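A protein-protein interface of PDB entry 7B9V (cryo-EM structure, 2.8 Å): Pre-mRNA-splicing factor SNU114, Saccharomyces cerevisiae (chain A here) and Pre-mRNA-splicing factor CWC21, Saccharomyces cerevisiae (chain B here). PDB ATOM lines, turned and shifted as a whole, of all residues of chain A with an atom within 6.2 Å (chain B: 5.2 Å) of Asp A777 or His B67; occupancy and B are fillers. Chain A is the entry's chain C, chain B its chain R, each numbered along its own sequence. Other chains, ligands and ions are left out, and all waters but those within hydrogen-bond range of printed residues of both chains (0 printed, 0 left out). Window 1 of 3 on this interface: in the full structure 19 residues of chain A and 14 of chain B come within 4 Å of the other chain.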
ATOM      1  N   LEU A 760       0.297 -13.458 -32.511  1.00  0.00           N
ATOM      2  CA  LEU A 760       0.278 -13.917 -31.129  1.00  0.00           C
ATOM      3  C   LEU A 760       1.065 -12.967 -30.236  1.00  0.00           C
ATOM      4  O   LEU A 760       0.533 -12.453 -29.250  1.00  0.00           O
ATOM      5  CB  LEU A 760       0.879 -15.320 -31.056  1.00  0.00           C
ATOM      6  CG  LEU A 760       1.129 -15.992 -29.712  1.00  0.00           C
ATOM      7  CD1 LEU A 760      -0.174 -16.151 -28.936  1.00  0.00           C
ATOM      8  CD2 LEU A 760       1.805 -17.307 -29.948  1.00  0.00           C
ATOM      9  N   ALA A 761       2.344 -12.728 -30.577  1.00  0.00           N
ATOM     10  CA  ALA A 761       3.157 -11.752 -29.853  1.00  0.00           C
ATOM     11  C   ALA A 761       2.607 -10.337 -29.977  1.00  0.00           C
ATOM     12  O   ALA A 761       2.830  -9.510 -29.083  1.00  0.00           O
ATOM     13  CB  ALA A 761       4.597 -11.791 -30.357  1.00  0.00           C
ATOM     14  N   SER A 762       1.982 -10.021 -31.124  1.00  0.00           N
ATOM     15  CA  SER A 762       1.441  -8.686 -31.365  1.00  0.00           C
ATOM     16  C   SER A 762       0.331  -8.351 -30.379  1.00  0.00           C
ATOM     17  O   SER A 762       0.234  -7.219 -29.895  1.00  0.00           O
ATOM     18  CB  SER A 762       0.941  -8.593 -32.803  1.00  0.00           C
ATOM     19  OG  SER A 762       0.448  -7.346 -33.148  1.00  0.00           O
ATOM     20  N   ASN A 764       0.037 -10.079 -27.472  1.00  0.00           N
ATOM     21  CA  ASN A 764       0.572 -10.397 -26.151  1.00  0.00           C
ATOM     22  C   ASN A 764       1.487  -9.332 -25.563  1.00  0.00           C
ATOM     23  O   ASN A 764       2.188  -9.635 -24.589  1.00  0.00           O
ATOM     24  CB  ASN A 764       1.312 -11.728 -26.173  1.00  0.00           C
ATOM     25  CG  ASN A 764       0.374 -12.911 -26.133  1.00  0.00           C
ATOM     26  OD1 ASN A 764      -0.795 -12.787 -25.763  1.00  0.00           O
ATOM     27  ND2 ASN A 764       0.897 -14.080 -26.471  1.00  0.00           N
ATOM     28  N   ILE A 775       6.501  -8.943 -23.375  1.00  0.00           N
ATOM     29  CA  ILE A 775       5.535  -9.737 -24.123  1.00  0.00           C
ATOM     30  C   ILE A 775       5.204 -10.936 -23.260  1.00  0.00           C
ATOM     31  O   ILE A 775       6.096 -11.716 -22.907  1.00  0.00           O
ATOM     32  CB  ILE A 775       6.052 -10.196 -25.499  1.00  0.00           C
ATOM     33  CG1 ILE A 775       6.714  -9.061 -26.281  1.00  0.00           C
ATOM     34  CG2 ILE A 775       4.925 -10.786 -26.318  1.00  0.00           C
ATOM     35  CD1 ILE A 775       7.474  -9.544 -27.484  1.00  0.00           C
ATOM     36  N   ASN A 776       3.928 -11.095 -22.928  1.00  0.00           N
ATOM     37  CA  ASN A 776       3.485 -12.262 -22.173  1.00  0.00           C
ATOM     38  C   ASN A 776       3.022 -13.343 -23.146  1.00  0.00           C
ATOM     39  O   ASN A 776       1.832 -13.496 -23.426  1.00  0.00           O
ATOM     40  CB  ASN A 776       2.405 -11.840 -21.179  1.00  0.00           C
ATOM     41  CG  ASN A 776       2.102 -12.899 -20.122  1.00  0.00           C
ATOM     42  OD1 ASN A 776       2.202 -14.061 -20.358  1.00  0.00           O
ATOM     43  ND2 ASN A 776       1.792 -12.458 -18.930  1.00  0.00           N
ATOM     44  N   ASP A 777       3.976 -14.157 -23.600  1.00  0.00           N
ATOM     45  CA  ASP A 777       3.696 -15.379 -24.343  1.00  0.00           C
ATOM     46  C   ASP A 777       3.535 -16.623 -23.455  1.00  0.00           C
ATOM     47  O   ASP A 777       3.882 -17.719 -23.920  1.00  0.00           O
ATOM     48  CB  ASP A 777       4.788 -15.617 -25.387  1.00  0.00           C
ATOM     49  CG  ASP A 777       4.781 -14.578 -26.485  1.00  0.00           C
ATOM     50  OD1 ASP A 777       3.689 -14.067 -26.817  1.00  0.00           O
ATOM     51  OD2 ASP A 777       5.869 -14.265 -27.014  1.00  0.00           O
ATOM     52  N   THR A 778       3.154 -16.470 -22.173  1.00  0.00           N
ATOM     53  CA  THR A 778       2.850 -17.617 -21.304  1.00  0.00           C
ATOM     54  C   THR A 778       1.745 -18.467 -21.919  1.00  0.00           C
ATOM     55  O   THR A 778       0.694 -17.957 -22.316  1.00  0.00           O
ATOM     56  CB  THR A 778       2.439 -17.179 -19.880  1.00  0.00           C
ATOM     57  OG1 THR A 778       3.470 -16.401 -19.292  1.00  0.00           O
ATOM     58  CG2 THR A 778       2.126 -18.364 -18.949  1.00  0.00           C
ATOM     59  N   LEU A 779       1.985 -19.746 -21.991  1.00  0.00           N
ATOM     60  CA  LEU A 779       1.059 -20.652 -22.629  1.00  0.00           C
ATOM     61  C   LEU A 779      -0.083 -20.949 -21.661  1.00  0.00           C
ATOM     62  O   LEU A 779       0.139 -21.008 -20.449  1.00  0.00           O
ATOM     63  CB  LEU A 779       1.792 -21.932 -22.994  1.00  0.00           C
ATOM     64  CG  LEU A 779       2.802 -21.732 -24.117  1.00  0.00           C
ATOM     65  CD1 LEU A 779       3.767 -22.891 -24.101  1.00  0.00           C
ATOM     66  CD2 LEU A 779       2.097 -21.630 -25.464  1.00  0.00           C
ATOM     67  N   LYS A 819      10.311 -11.924 -23.070  1.00  0.00           N
ATOM     68  CA  LYS A 819       9.254 -12.896 -23.319  1.00  0.00           C
ATOM     69  C   LYS A 819       9.089 -13.793 -22.105  1.00  0.00           C
ATOM     70  O   LYS A 819      10.029 -14.489 -21.717  1.00  0.00           O
ATOM     71  CB  LYS A 819       9.563 -13.736 -24.559  1.00  0.00           C
ATOM     72  CG  LYS A 819       9.613 -12.938 -25.844  1.00  0.00           C
ATOM     73  CD  LYS A 819       9.826 -13.839 -27.047  1.00  0.00           C
ATOM     74  CE  LYS A 819      11.221 -14.443 -27.052  1.00  0.00           C
ATOM     75  NZ  LYS A 819      11.618 -14.896 -28.413  1.00  0.00           N
ATOM     76  N   LEU A 820       7.882 -13.815 -21.546  1.00  0.00           N
ATOM     77  CA  LEU A 820       7.541 -14.748 -20.482  1.00  0.00           C
ATOM     78  C   LEU A 820       7.329 -16.141 -21.058  1.00  0.00           C
ATOM     79  O   LEU A 820       6.619 -16.314 -22.053  1.00  0.00           O
ATOM     80  CB  LEU A 820       6.287 -14.293 -19.731  1.00  0.00           C
ATOM     81  CG  LEU A 820       6.429 -13.372 -18.516  1.00  0.00           C
ATOM     82  CD1 LEU A 820       5.176 -12.556 -18.317  1.00  0.00           C
ATOM     83  CD2 LEU A 820       6.675 -14.207 -17.270  1.00  0.00           C
ATOM     84  N   LEU A 821       7.940 -17.133 -20.411  1.00  0.00           N
ATOM     85  CA  LEU A 821       7.605 -18.531 -20.656  1.00  0.00           C
ATOM     86  C   LEU A 821       6.478 -18.989 -19.737  1.00  0.00           C
ATOM     87  O   LEU A 821       5.437 -19.432 -20.236  1.00  0.00           O
ATOM     88  CB  LEU A 821       8.842 -19.424 -20.477  1.00  0.00           C
ATOM     89  CG  LEU A 821       8.634 -20.945 -20.606  1.00  0.00           C
ATOM     90  CD1 LEU A 821       8.007 -21.339 -21.921  1.00  0.00           C
ATOM     91  CD2 LEU A 821       9.947 -21.692 -20.445  1.00  0.00           C
ATOM     92  N   LYS B  62      16.495 -27.764 -23.854  1.00  0.00           N
ATOM     93  CA  LYS B  62      15.397 -28.407 -24.579  1.00  0.00           C
ATOM     94  C   LYS B  62      14.048 -27.719 -24.341  1.00  0.00           C
ATOM     95  O   LYS B  62      13.114 -27.920 -25.126  1.00  0.00           O
ATOM     96  CB  LYS B  62      15.333 -29.894 -24.180  1.00  0.00           C
ATOM     97  CG  LYS B  62      14.491 -30.806 -25.083  1.00  0.00           C
ATOM     98  CD  LYS B  62      14.599 -32.276 -24.751  1.00  0.00           C
ATOM     99  CE  LYS B  62      13.799 -33.075 -25.757  1.00  0.00           C
ATOM    100  NZ  LYS B  62      13.934 -34.521 -25.492  1.00  0.00           N
ATOM    101  N   GLN B  63      13.942 -26.865 -23.312  1.00  0.00           N
ATOM    102  CA  GLN B  63      12.661 -26.245 -23.000  1.00  0.00           C
ATOM    103  C   GLN B  63      12.256 -25.208 -24.043  1.00  0.00           C
ATOM    104  O   GLN B  63      11.058 -24.969 -24.225  1.00  0.00           O
ATOM    105  CB  GLN B  63      12.710 -25.643 -21.599  1.00  0.00           C
ATOM    106  CG  GLN B  63      12.898 -26.707 -20.527  1.00  0.00           C
ATOM    107  CD  GLN B  63      12.750 -26.168 -19.125  1.00  0.00           C
ATOM    108  OE1 GLN B  63      12.923 -24.975 -18.886  1.00  0.00           O
ATOM    109  NE2 GLN B  63      12.421 -27.047 -18.184  1.00  0.00           N
ATOM    110  N   ILE B  64      13.232 -24.540 -24.685  1.00  0.00           N
ATOM    111  CA  ILE B  64      12.919 -23.689 -25.835  1.00  0.00           C
ATOM    112  C   ILE B  64      12.326 -24.534 -26.961  1.00  0.00           C
ATOM    113  O   ILE B  64      11.328 -24.149 -27.601  1.00  0.00           O
ATOM    114  CB  ILE B  64      14.181 -22.915 -26.273  1.00  0.00           C
ATOM    115  CG1 ILE B  64      14.568 -21.883 -25.211  1.00  0.00           C
ATOM    116  CG2 ILE B  64      14.016 -22.235 -27.625  1.00  0.00           C
ATOM    117  CD1 ILE B  64      15.946 -21.326 -25.395  1.00  0.00           C
ATOM    118  N   GLU B  65      12.949 -25.704 -27.215  1.00  0.00           N
ATOM    119  CA  GLU B  65      12.481 -26.632 -28.242  1.00  0.00           C
ATOM    120  C   GLU B  65      11.087 -27.155 -27.927  1.00  0.00           C
ATOM    121  O   GLU B  65      10.301 -27.421 -28.842  1.00  0.00           O
ATOM    122  CB  GLU B  65      13.463 -27.800 -28.398  1.00  0.00           C
ATOM    123  CG  GLU B  65      14.921 -27.425 -28.703  1.00  0.00           C
ATOM    124  CD  GLU B  65      15.205 -26.986 -30.150  1.00  0.00           C
ATOM    125  OE1 GLU B  65      14.277 -26.732 -30.955  1.00  0.00           O
ATOM    126  OE2 GLU B  65      16.403 -26.892 -30.488  1.00  0.00           O
ATOM    127  N   THR B  66      10.774 -27.303 -26.635  1.00  0.00           N
ATOM    128  CA  THR B  66       9.420 -27.655 -26.229  1.00  0.00           C
ATOM    129  C   THR B  66       8.467 -26.497 -26.480  1.00  0.00           C
ATOM    130  O   THR B  66       7.337 -26.706 -26.948  1.00  0.00           O
ATOM    131  CB  THR B  66       9.419 -28.048 -24.748  1.00  0.00           C
ATOM    132  OG1 THR B  66      10.355 -29.110 -24.533  1.00  0.00           O
ATOM    133  CG2 THR B  66       8.038 -28.508 -24.282  1.00  0.00           C
ATOM    134  N   HIS B  67       8.916 -25.269 -26.163  1.00  0.00           N
ATOM    135  CA  HIS B  67       8.056 -24.092 -26.263  1.00  0.00           C
ATOM    136  C   HIS B  67       7.640 -23.793 -27.696  1.00  0.00           C
ATOM    137  O   HIS B  67       6.549 -23.250 -27.906  1.00  0.00           O
ATOM    138  CB  HIS B  67       8.764 -22.886 -25.627  1.00  0.00           C
ATOM    139  CG  HIS B  67       8.020 -21.589 -25.766  1.00  0.00           C
ATOM    140  ND1 HIS B  67       6.862 -21.321 -25.072  1.00  0.00           N
ATOM    141  CD2 HIS B  67       8.317 -20.459 -26.453  1.00  0.00           C
ATOM    142  CE1 HIS B  67       6.446 -20.102 -25.364  1.00  0.00           C
ATOM    143  NE2 HIS B  67       7.315 -19.554 -26.193  1.00  0.00           N
ATOM    144  N   MET B  68       8.497 -24.128 -28.683  1.00  0.00           N
ATOM    145  CA  MET B  68       8.171 -23.820 -30.081  1.00  0.00           C
ATOM    146  C   MET B  68       6.922 -24.558 -30.572  1.00  0.00           C
ATOM    147  O   MET B  68       6.087 -23.975 -31.294  1.00  0.00           O
ATOM    148  CB  MET B  68       9.371 -24.152 -30.966  1.00  0.00           C
ATOM    149  CG  MET B  68      10.583 -23.238 -30.782  1.00  0.00           C
ATOM    150  SD  MET B  68      10.351 -21.570 -31.439  1.00  0.00           S
ATOM    151  CE  MET B  68      10.044 -20.601 -29.957  1.00  0.00           C
ATOM    152  N   GLU B  69       6.826 -25.864 -30.251  1.00  0.00           N
ATOM    153  CA  GLU B  69       5.728 -26.678 -30.766  1.00  0.00           C
ATOM    154  C   GLU B  69       4.391 -26.210 -30.207  1.00  0.00           C
ATOM    155  O   GLU B  69       3.379 -26.193 -30.916  1.00  0.00           O
ATOM    156  CB  GLU B  69       5.966 -28.155 -30.431  1.00  0.00           C
ATOM    157  CG  GLU B  69       4.887 -29.134 -30.932  1.00  0.00           C
ATOM    158  CD  GLU B  69       3.826 -29.480 -29.894  1.00  0.00           C
ATOM    159  OE1 GLU B  69       4.014 -29.154 -28.704  1.00  0.00           O
ATOM    160  OE2 GLU B  69       2.784 -30.045 -30.283  1.00  0.00           O
ATOM    161  N   LYS B  70       4.386 -25.791 -28.934  1.00  0.00           N
ATOM    162  CA  LYS B  70       3.191 -25.214 -28.344  1.00  0.00           C
ATOM    163  C   LYS B  70       2.951 -23.778 -28.783  1.00  0.00           C
ATOM    164  O   LYS B  70       1.822 -23.296 -28.644  1.00  0.00           O
ATOM    165  CB  LYS B  70       3.263 -25.318 -26.824  1.00  0.00           C
ATOM    166  CG  LYS B  70       3.174 -26.749 -26.312  1.00  0.00           C
ATOM    167  CD  LYS B  70       2.817 -26.794 -24.838  1.00  0.00           C
ATOM    168  CE  LYS B  70       2.521 -28.219 -24.403  1.00  0.00           C
ATOM    169  NZ  LYS B  70       1.902 -28.292 -23.051  1.00  0.00           N
ATOM    170  N   ARG B  71       3.995 -23.069 -29.245  1.00  0.00           N
ATOM    171  CA  ARG B  71       3.790 -21.746 -29.831  1.00  0.00           C
ATOM    172  C   ARG B  71       2.965 -21.826 -31.095  1.00  0.00           C
ATOM    173  O   ARG B  71       2.121 -20.951 -31.328  1.00  0.00           O
ATOM    174  CB  ARG B  71       5.112 -21.042 -30.154  1.00  0.00           C
ATOM    175  CG  ARG B  71       5.740 -20.256 -29.025  1.00  0.00           C
ATOM    176  CD  ARG B  71       4.983 -18.968 -28.697  1.00  0.00           C
ATOM    177  NE  ARG B  71       5.088 -17.976 -29.763  1.00  0.00           N
ATOM    178  CZ  ARG B  71       5.780 -16.848 -29.676  1.00  0.00           C
ATOM    179  NH1 ARG B  71       6.438 -16.525 -28.576  1.00  0.00           N
ATOM    180  NH2 ARG B  71       5.812 -16.027 -30.721  1.00  0.00           N
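The guanidinium group (NH1) of Arg B71 lies within salt-bridge range of the side-chain carboxylate (OD2) of Asp A777.
The side-chain amide nitrogen (ND2) of Asn A764 lies close to the backbone carbonyl oxygen (O) of Leu A760, at 3.2 Å. The side-chain amide nitrogen of Asn A764 is in hydrogen-bond range of the side-chain carboxylate of Asp A777 (2.8 Å).
Among the printed residues, pairs that only touch across the chains: Leu A821 with His B67 (3.4 Å), Leu A760 with Arg B71 (3.4 Å), Leu A779 with Lys B70 (3.6 Å), Leu A779 with His B67 (3.6 Å) and Asp A777 with His B67 (3.8 Å).
Of the printed residues of chain B, Leu A760 touches Arg B71. Of the printed residues of chain B, Asp A777 touches His B67 (3.8 Å) and Arg B71 (2.8 Å). Printed residues of chain B within 4 Å of Leu A779: His B67 (3.6 Å) and Lys B70 (3.6 Å). Printed residues of chain B within 4 Å of Leu A821: His B67 (3.4 Å). Thr B66 touches none of the printed residues of chain A. His B67 touches just these residues of chain A: Asp A777, Leu A779 and Leu A821. Met B68 touches none of the printed residues of chain A. Printed residues of chain A within 4 Å of Lys B70: Leu A779. The nearest printed residue of chain A that does not touch Arg B71 is Ala A761 (4.4 Å).
Of the 10 printed residues of chain B, 3 touch a printed residue of chain A. Hydrophobic or aromatic side chains of chain A that line the printed part of chain B: Leu A760, Leu A779 and Leu A821. Among the printed residues, 6 pairs touch across the chains. Among the printed residues, Asp or Glu carboxylates within 4 Å of a Lys or Arg side-chain nitrogen of the other chain: Asp A777 with Arg B71.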
